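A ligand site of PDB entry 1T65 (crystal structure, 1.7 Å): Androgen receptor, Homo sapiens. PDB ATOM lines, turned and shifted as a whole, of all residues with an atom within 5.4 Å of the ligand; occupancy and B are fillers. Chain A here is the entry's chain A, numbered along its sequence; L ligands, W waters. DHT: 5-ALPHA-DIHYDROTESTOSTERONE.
Water W1 lies within hydrogen-bond range of the side-chain amide nitrogen (NE2) of Gln 43 (2.6 Å), the backbone carbonyl oxygen (O) of Met 77 (2.8 Å), the guanidinium group (NH2) of Arg 84 (3.0 Å) and an oxygen (O3) of the ligand (3.4 Å).
Leu 33 touches the ligand.
O of Leu 36 touches C11 of the ligand, 3.4 Å away.
CD2 of Leu 39 touches C2 of the ligand, at 3.98 Å.
Gln 43 touches the ligand (NE2 to C2, 3.3 Å).
Met 74 touches the ligand.
Met 77 touches the ligand.
Met 81 touches the ligand (CB to O3, 3.7 Å).
Phe 96 touches the ligand (CE1 to C5, 3.8 Å).
Met 112 touches the ligand (CE to C16, 3.7 Å).
CD1 of Phe 208 touches C16 of the ligand, at 3.8 Å.
Met 227 touches the ligand.
Hydrophobic or aromatic side chains within 4 Å of the ligand: Leu 33, Leu 39, Met 74, Met 77, Met 81, Phe 96, Met 112, Phe 208 and Met 227.
Within 4 Å of the ligand: Leu 33, Leu 36, Asn 37, Leu 39, Gln 43, Met 74, Met 77, Met 81, Arg 84, Phe 96, Met 112, Phe 208, Thr 209 and Met 227.
The nearest printed residue that does not touch the ligand is Phe 223 (4.05 Å).
The side-chain hydroxyl (OG1) of Thr 209 lies within hydrogen-bond range of an oxygen (O17) of the ligand, 2.7 Å away.
OD1 of Asn 37 sits at hydrogen-bond distance from O17 of the ligand (2.8 Å).
NH2 of Arg 84 is in hydrogen-bond range of O3 of the ligand (3.1 Å).
The backbone carbonyl oxygen of Leu 33 sits close to the side-chain amide nitrogen of Asn 37, 3.5 Å away.
OE1 of Gln 43 is in hydrogen-bond range of NH2 of Arg 84 (3.5 Å).
The backbone carbonyl oxygen (O) of Phe 96 lies within hydrogen-bond range of the guanidinium group (NH2) of Arg 84 (3.0 Å).
NE2 of Gln 43 lies close to SD of Met 77, at 3.6 Å.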
ATOM      1  N   LEU A  33      25.200  31.318   9.603  1.00  0.00           N
ATOM      2  CA  LEU A  33      24.187  31.577   8.587  1.00  0.00           C
ATOM      3  C   LEU A  33      24.740  32.307   7.377  1.00  0.00           C
ATOM      4  O   LEU A  33      24.332  32.051   6.241  1.00  0.00           O
ATOM      5  CB  LEU A  33      22.988  32.342   9.185  1.00  0.00           C
ATOM      6  CG  LEU A  33      21.825  31.464   9.671  1.00  0.00           C
ATOM      7  CD1 LEU A  33      21.245  30.677   8.475  1.00  0.00           C
ATOM      8  CD2 LEU A  33      22.315  30.505  10.749  1.00  0.00           C
ATOM      9  N   LEU A  36      26.321  29.656   5.280  1.00  0.00           N
ATOM     10  CA  LEU A  36      25.335  28.826   4.601  1.00  0.00           C
ATOM     11  C   LEU A  36      24.800  29.582   3.389  1.00  0.00           C
ATOM     12  O   LEU A  36      24.621  28.990   2.320  1.00  0.00           O
ATOM     13  CB  LEU A  36      24.191  28.459   5.550  1.00  0.00           C
ATOM     14  CG  LEU A  36      24.483  27.322   6.543  1.00  0.00           C
ATOM     15  CD1 LEU A  36      23.377  27.252   7.589  1.00  0.00           C
ATOM     16  CD2 LEU A  36      24.580  25.996   5.789  1.00  0.00           C
ATOM     17  N   ASN A  37      24.575  30.881   3.543  1.00  0.00           N
ATOM     18  CA  ASN A  37      24.090  31.701   2.425  1.00  0.00           C
ATOM     19  C   ASN A  37      25.107  31.765   1.281  1.00  0.00           C
ATOM     20  O   ASN A  37      24.723  31.711   0.110  1.00  0.00           O
ATOM     21  CB  ASN A  37      23.765  33.128   2.895  1.00  0.00           C
ATOM     22  CG  ASN A  37      22.479  33.215   3.703  1.00  0.00           C
ATOM     23  OD1 ASN A  37      21.615  32.345   3.609  1.00  0.00           O
ATOM     24  ND2 ASN A  37      22.336  34.291   4.478  1.00  0.00           N
ATOM     25  N   LEU A  39      27.405  29.492   0.628  1.00  0.00           N
ATOM     26  CA  LEU A  39      27.461  28.149   0.049  1.00  0.00           C
ATOM     27  C   LEU A  39      26.285  28.013  -0.912  1.00  0.00           C
ATOM     28  O   LEU A  39      26.391  27.381  -1.953  1.00  0.00           O
ATOM     29  CB  LEU A  39      27.366  27.068   1.136  1.00  0.00           C
ATOM     30  CG  LEU A  39      27.322  25.615   0.643  1.00  0.00           C
ATOM     31  CD1 LEU A  39      28.624  25.258  -0.065  1.00  0.00           C
ATOM     32  CD2 LEU A  39      27.108  24.685   1.829  1.00  0.00           C
ATOM     33  N   GLY A  40      25.151  28.613  -0.546  1.00  0.00           N
ATOM     34  CA  GLY A  40      23.977  28.552  -1.392  1.00  0.00           C
ATOM     35  C   GLY A  40      24.242  29.241  -2.721  1.00  0.00           C
ATOM     36  O   GLY A  40      23.898  28.723  -3.790  1.00  0.00           O
ATOM     37  N   GLN A  43      26.637  27.084  -4.747  1.00  0.00           N
ATOM     38  CA  GLN A  43      26.000  25.889  -5.251  1.00  0.00           C
ATOM     39  C   GLN A  43      25.019  26.226  -6.369  1.00  0.00           C
ATOM     40  O   GLN A  43      24.822  25.429  -7.285  1.00  0.00           O
ATOM     41  CB  GLN A  43      25.282  25.120  -4.125  1.00  0.00           C
ATOM     42  CG  GLN A  43      26.239  24.502  -3.114  1.00  0.00           C
ATOM     43  CD  GLN A  43      25.655  23.306  -2.378  1.00  0.00           C
ATOM     44  OE1 GLN A  43      26.315  22.708  -1.523  1.00  0.00           O
ATOM     45  NE2 GLN A  43      24.416  22.950  -2.713  1.00  0.00           N
ATOM     46  N   TRP A  73      15.504  24.741  -6.315  1.00  0.00           N
ATOM     47  CA  TRP A  73      16.869  24.693  -5.787  1.00  0.00           C
ATOM     48  C   TRP A  73      16.986  24.227  -4.339  1.00  0.00           C
ATOM     49  O   TRP A  73      17.906  23.465  -4.015  1.00  0.00           O
ATOM     50  CB  TRP A  73      17.563  26.049  -5.947  1.00  0.00           C
ATOM     51  CG  TRP A  73      16.917  27.171  -5.204  1.00  0.00           C
ATOM     52  CD1 TRP A  73      15.900  27.960  -5.641  1.00  0.00           C
ATOM     53  CD2 TRP A  73      17.217  27.603  -3.866  1.00  0.00           C
ATOM     54  NE1 TRP A  73      15.542  28.864  -4.654  1.00  0.00           N
ATOM     55  CE2 TRP A  73      16.338  28.658  -3.566  1.00  0.00           C
ATOM     56  CE3 TRP A  73      18.158  27.200  -2.898  1.00  0.00           C
ATOM     57  CZ2 TRP A  73      16.357  29.321  -2.327  1.00  0.00           C
ATOM     58  CZ3 TRP A  73      18.175  27.851  -1.672  1.00  0.00           C
ATOM     59  CH2 TRP A  73      17.279  28.908  -1.396  1.00  0.00           C
ATOM     60  N   MET A  74      16.077  24.648  -3.461  1.00  0.00           N
ATOM     61  CA  MET A  74      16.155  24.244  -2.054  1.00  0.00           C
ATOM     62  C   MET A  74      16.061  22.719  -1.916  1.00  0.00           C
ATOM     63  O   MET A  74      16.899  22.103  -1.263  1.00  0.00           O
ATOM     64  CB  MET A  74      15.041  24.920  -1.229  1.00  0.00           C
ATOM     65  CG  MET A  74      15.106  24.648   0.286  1.00  0.00           C
ATOM     66  SD  MET A  74      16.480  25.452   1.155  1.00  0.00           S
ATOM     67  CE  MET A  74      15.788  27.114   1.427  1.00  0.00           C
ATOM     68  N   MET A  77      19.268  20.945  -3.401  1.00  0.00           N
ATOM     69  CA  MET A  77      20.436  21.064  -2.547  1.00  0.00           C
ATOM     70  C   MET A  77      20.332  20.276  -1.242  1.00  0.00           C
ATOM     71  O   MET A  77      21.330  19.742  -0.756  1.00  0.00           O
ATOM     72  CB  MET A  77      20.717  22.543  -2.244  1.00  0.00           C
ATOM     73  CG  MET A  77      21.059  23.350  -3.481  1.00  0.00           C
ATOM     74  SD  MET A  77      21.462  25.060  -3.084  1.00  0.00           S
ATOM     75  CE  MET A  77      21.499  25.791  -4.727  1.00  0.00           C
ATOM     76  N   VAL A  78      19.129  20.200  -0.680  1.00  0.00           N
ATOM     77  CA  VAL A  78      18.923  19.449   0.553  1.00  0.00           C
ATOM     78  C   VAL A  78      19.107  17.950   0.287  1.00  0.00           C
ATOM     79  O   VAL A  78      19.728  17.246   1.074  1.00  0.00           O
ATOM     80  CB  VAL A  78      17.520  19.717   1.153  1.00  0.00           C
ATOM     81  CG1 VAL A  78      17.218  18.730   2.261  1.00  0.00           C
ATOM     82  CG2 VAL A  78      17.462  21.134   1.715  1.00  0.00           C
ATOM     83  N   MET A  81      22.772  17.206  -0.188  1.00  0.00           N
ATOM     84  CA  MET A  81      23.478  17.330   1.093  1.00  0.00           C
ATOM     85  C   MET A  81      23.244  16.083   1.932  1.00  0.00           C
ATOM     86  O   MET A  81      24.151  15.600   2.622  1.00  0.00           O
ATOM     87  CB  MET A  81      22.993  18.585   1.832  1.00  0.00           C
ATOM     88  CG  MET A  81      23.767  18.921   3.108  1.00  0.00           C
ATOM     89  SD  MET A  81      23.199  18.023   4.559  1.00  0.00           S
ATOM     90  CE  MET A  81      21.575  18.768   4.806  1.00  0.00           C
ATOM     91  N   ARG A  84      25.518  13.361   0.604  1.00  0.00           N
ATOM     92  CA  ARG A  84      26.918  13.601   0.998  1.00  0.00           C
ATOM     93  C   ARG A  84      27.129  13.207   2.448  1.00  0.00           C
ATOM     94  O   ARG A  84      28.162  12.636   2.807  1.00  0.00           O
ATOM     95  CB  ARG A  84      27.295  15.081   0.853  1.00  0.00           C
ATOM     96  CG  ARG A  84      27.455  15.601  -0.553  1.00  0.00           C
ATOM     97  CD  ARG A  84      28.222  16.924  -0.558  1.00  0.00           C
ATOM     98  NE  ARG A  84      27.498  18.024   0.078  1.00  0.00           N
ATOM     99  CZ  ARG A  84      26.511  18.711  -0.500  1.00  0.00           C
ATOM    100  NH1 ARG A  84      26.137  18.422  -1.748  1.00  0.00           N
ATOM    101  NH2 ARG A  84      25.917  19.709   0.146  1.00  0.00           N
ATOM    102  N   PHE A  96      27.323  19.872   4.915  1.00  0.00           N
ATOM    103  CA  PHE A  96      26.968  20.923   3.971  1.00  0.00           C
ATOM    104  C   PHE A  96      28.103  21.097   2.963  1.00  0.00           C
ATOM    105  O   PHE A  96      27.862  21.267   1.772  1.00  0.00           O
ATOM    106  CB  PHE A  96      26.695  22.239   4.714  1.00  0.00           C
ATOM    107  CG  PHE A  96      25.424  22.225   5.539  1.00  0.00           C
ATOM    108  CD1 PHE A  96      24.174  22.288   4.918  1.00  0.00           C
ATOM    109  CD2 PHE A  96      25.471  22.132   6.922  1.00  0.00           C
ATOM    110  CE1 PHE A  96      22.993  22.247   5.665  1.00  0.00           C
ATOM    111  CE2 PHE A  96      24.294  22.094   7.691  1.00  0.00           C
ATOM    112  CZ  PHE A  96      23.062  22.159   7.058  1.00  0.00           C
ATOM    113  N   MET A 112      17.812  26.627  13.735  1.00  0.00           N
ATOM    114  CA  MET A 112      16.915  25.851  12.886  1.00  0.00           C
ATOM    115  C   MET A 112      17.176  24.375  13.207  1.00  0.00           C
ATOM    116  O   MET A 112      17.313  23.533  12.334  1.00  0.00           O
ATOM    117  CB  MET A 112      17.149  26.142  11.395  1.00  0.00           C
ATOM    118  CG  MET A 112      18.533  25.884  10.871  1.00  0.00           C
ATOM    119  SD  MET A 112      18.589  26.165   9.063  1.00  0.00           S
ATOM    120  CE  MET A 112      19.609  27.613   8.964  1.00  0.00           C
ATOM    121  N   MET A 119      16.621  16.805   8.407  1.00  0.00           N
ATOM    122  CA  MET A 119      17.521  16.570   7.281  1.00  0.00           C
ATOM    123  C   MET A 119      18.459  15.400   7.605  1.00  0.00           C
ATOM    124  O   MET A 119      18.920  14.690   6.711  1.00  0.00           O
ATOM    125  CB  MET A 119      18.336  17.827   6.953  1.00  0.00           C
ATOM    126  CG  MET A 119      17.501  18.963   6.357  1.00  0.00           C
ATOM    127  SD  MET A 119      18.461  20.360   5.730  1.00  0.00           S
ATOM    128  CE  MET A 119      18.786  21.251   7.251  1.00  0.00           C
ATOM    129  N   LEU A 205      12.341  25.307   5.424  1.00  0.00           N
ATOM    130  CA  LEU A 205      13.544  26.097   5.196  1.00  0.00           C
ATOM    131  C   LEU A 205      13.184  27.353   4.410  1.00  0.00           C
ATOM    132  O   LEU A 205      13.785  28.409   4.620  1.00  0.00           O
ATOM    133  CB  LEU A 205      14.592  25.255   4.452  1.00  0.00           C
ATOM    134  CG  LEU A 205      15.167  24.084   5.266  1.00  0.00           C
ATOM    135  CD1 LEU A 205      16.003  23.168   4.382  1.00  0.00           C
ATOM    136  CD2 LEU A 205      15.994  24.640   6.426  1.00  0.00           C
ATOM    137  N   PHE A 208      11.934  29.717   6.946  1.00  0.00           N
ATOM    138  CA  PHE A 208      13.038  30.183   7.779  1.00  0.00           C
ATOM    139  C   PHE A 208      13.922  31.217   7.087  1.00  0.00           C
ATOM    140  O   PHE A 208      14.238  32.255   7.669  1.00  0.00           O
ATOM    141  CB  PHE A 208      13.889  28.994   8.236  1.00  0.00           C
ATOM    142  CG  PHE A 208      14.973  29.352   9.209  1.00  0.00           C
ATOM    143  CD1 PHE A 208      16.281  29.564   8.781  1.00  0.00           C
ATOM    144  CD2 PHE A 208      14.683  29.482  10.568  1.00  0.00           C
ATOM    145  CE1 PHE A 208      17.282  29.910   9.688  1.00  0.00           C
ATOM    146  CE2 PHE A 208      15.690  29.826  11.484  1.00  0.00           C
ATOM    147  CZ  PHE A 208      16.986  30.041  11.040  1.00  0.00           C
ATOM    148  N   THR A 209      14.332  30.932   5.849  1.00  0.00           N
ATOM    149  CA  THR A 209      15.198  31.863   5.149  1.00  0.00           C
ATOM    150  C   THR A 209      14.435  33.147   4.797  1.00  0.00           C
ATOM    151  O   THR A 209      15.023  34.224   4.797  1.00  0.00           O
ATOM    152  CB  THR A 209      15.830  31.216   3.881  1.00  0.00           C
ATOM    153  OG1 THR A 209      16.939  32.022   3.426  1.00  0.00           O
ATOM    154  CG2 THR A 209      14.808  31.077   2.749  1.00  0.00           C
ATOM    155  N   LEU A 212      14.384  35.242   7.849  1.00  0.00           N
ATOM    156  CA  LEU A 212      15.746  35.711   8.106  1.00  0.00           C
ATOM    157  C   LEU A 212      16.124  36.880   7.207  1.00  0.00           C
ATOM    158  O   LEU A 212      16.754  37.827   7.657  1.00  0.00           O
ATOM    159  CB  LEU A 212      16.746  34.565   7.921  1.00  0.00           C
ATOM    160  CG  LEU A 212      18.220  34.885   8.196  1.00  0.00           C
ATOM    161  CD1 LEU A 212      18.381  35.458   9.596  1.00  0.00           C
ATOM    162  CD2 LEU A 212      19.058  33.603   8.052  1.00  0.00           C
ATOM    163  N   PHE A 223      23.327  38.273   2.896  1.00  0.00           N
ATOM    164  CA  PHE A 223      22.714  37.516   1.799  1.00  0.00           C
ATOM    165  C   PHE A 223      23.312  37.958   0.470  1.00  0.00           C
ATOM    166  O   PHE A 223      23.265  39.142   0.131  1.00  0.00           O
ATOM    167  CB  PHE A 223      21.195  37.728   1.727  1.00  0.00           C
ATOM    168  CG  PHE A 223      20.412  36.917   2.724  1.00  0.00           C
ATOM    169  CD1 PHE A 223      20.294  37.322   4.048  1.00  0.00           C
ATOM    170  CD2 PHE A 223      19.757  35.748   2.321  1.00  0.00           C
ATOM    171  CE1 PHE A 223      19.534  36.596   4.963  1.00  0.00           C
ATOM    172  CE2 PHE A 223      18.995  35.010   3.224  1.00  0.00           C
ATOM    173  CZ  PHE A 223      18.883  35.434   4.545  1.00  0.00           C
ATOM    174  N   MET A 227      20.855  35.009  -4.089  1.00  0.00           N
ATOM    175  CA  MET A 227      20.036  34.464  -3.018  1.00  0.00           C
ATOM    176  C   MET A 227      18.970  35.476  -2.577  1.00  0.00           C
ATOM    177  O   MET A 227      17.799  35.127  -2.431  1.00  0.00           O
ATOM    178  CB  MET A 227      20.908  34.074  -1.828  1.00  0.00           C
ATOM    179  CG  MET A 227      21.799  32.854  -2.053  1.00  0.00           C
ATOM    180  SD  MET A 227      20.907  31.271  -2.068  1.00  0.00           S
ATOM    181  CE  MET A 227      20.712  30.965  -0.336  1.00  0.00           C
ATOM    182  N   ILE A 231      14.918  34.714  -2.959  1.00  0.00           N
ATOM    183  CA  ILE A 231      14.150  34.603  -1.725  1.00  0.00           C
ATOM    184  C   ILE A 231      13.100  35.713  -1.545  1.00  0.00           C
ATOM    185  O   ILE A 231      12.129  35.523  -0.813  1.00  0.00           O
ATOM    186  CB  ILE A 231      15.104  34.556  -0.501  1.00  0.00           C
ATOM    187  CG1 ILE A 231      16.002  33.312  -0.610  1.00  0.00           C
ATOM    188  CG2 ILE A 231      14.305  34.502   0.797  1.00  0.00           C
ATOM    189  CD1 ILE A 231      17.150  33.259   0.391  1.00  0.00           C
HETATM  190  C1  DHT L   1      23.085  25.347   1.149  1.00  0.00           C
HETATM  191  C2  DHT L   1      23.498  24.166   0.247  1.00  0.00           C
HETATM  192  C3  DHT L   1      23.228  22.863   1.057  1.00  0.00           C
HETATM  193  O3  DHT L   1      24.121  22.026   1.148  1.00  0.00           O
HETATM  194  C4  DHT L   1      21.883  22.717   1.714  1.00  0.00           C
HETATM  195  C5  DHT L   1      21.548  23.937   2.639  1.00  0.00           C
HETATM  196  C6  DHT L   1      20.146  23.818   3.326  1.00  0.00           C
HETATM  197  C7  DHT L   1      19.913  25.041   4.240  1.00  0.00           C
HETATM  198  C8  DHT L   1      19.981  26.395   3.467  1.00  0.00           C
HETATM  199  C9  DHT L   1      21.377  26.500   2.746  1.00  0.00           C
HETATM  200  C10 DHT L   1      21.660  25.279   1.771  1.00  0.00           C
HETATM  201  C11 DHT L   1      21.438  27.873   2.004  1.00  0.00           C
HETATM  202  C12 DHT L   1      21.169  29.129   2.848  1.00  0.00           C
HETATM  203  C13 DHT L   1      19.865  29.020   3.676  1.00  0.00           C
HETATM  204  C14 DHT L   1      19.822  27.626   4.403  1.00  0.00           C
HETATM  205  C15 DHT L   1      18.518  27.733   5.226  1.00  0.00           C
HETATM  206  C16 DHT L   1      18.633  29.174   5.803  1.00  0.00           C
HETATM  207  C17 DHT L   1      19.708  29.883   4.921  1.00  0.00           C
HETATM  208  O17 DHT L   1      19.272  31.227   4.639  1.00  0.00           O
HETATM  209  C18 DHT L   1      18.629  29.209   2.700  1.00  0.00           C
HETATM  210  C19 DHT L   1      20.587  25.286   0.615  1.00  0.00           C
HETATM  211  O   HOH W   1      23.801  20.509  -1.896  1.00  0.00           O
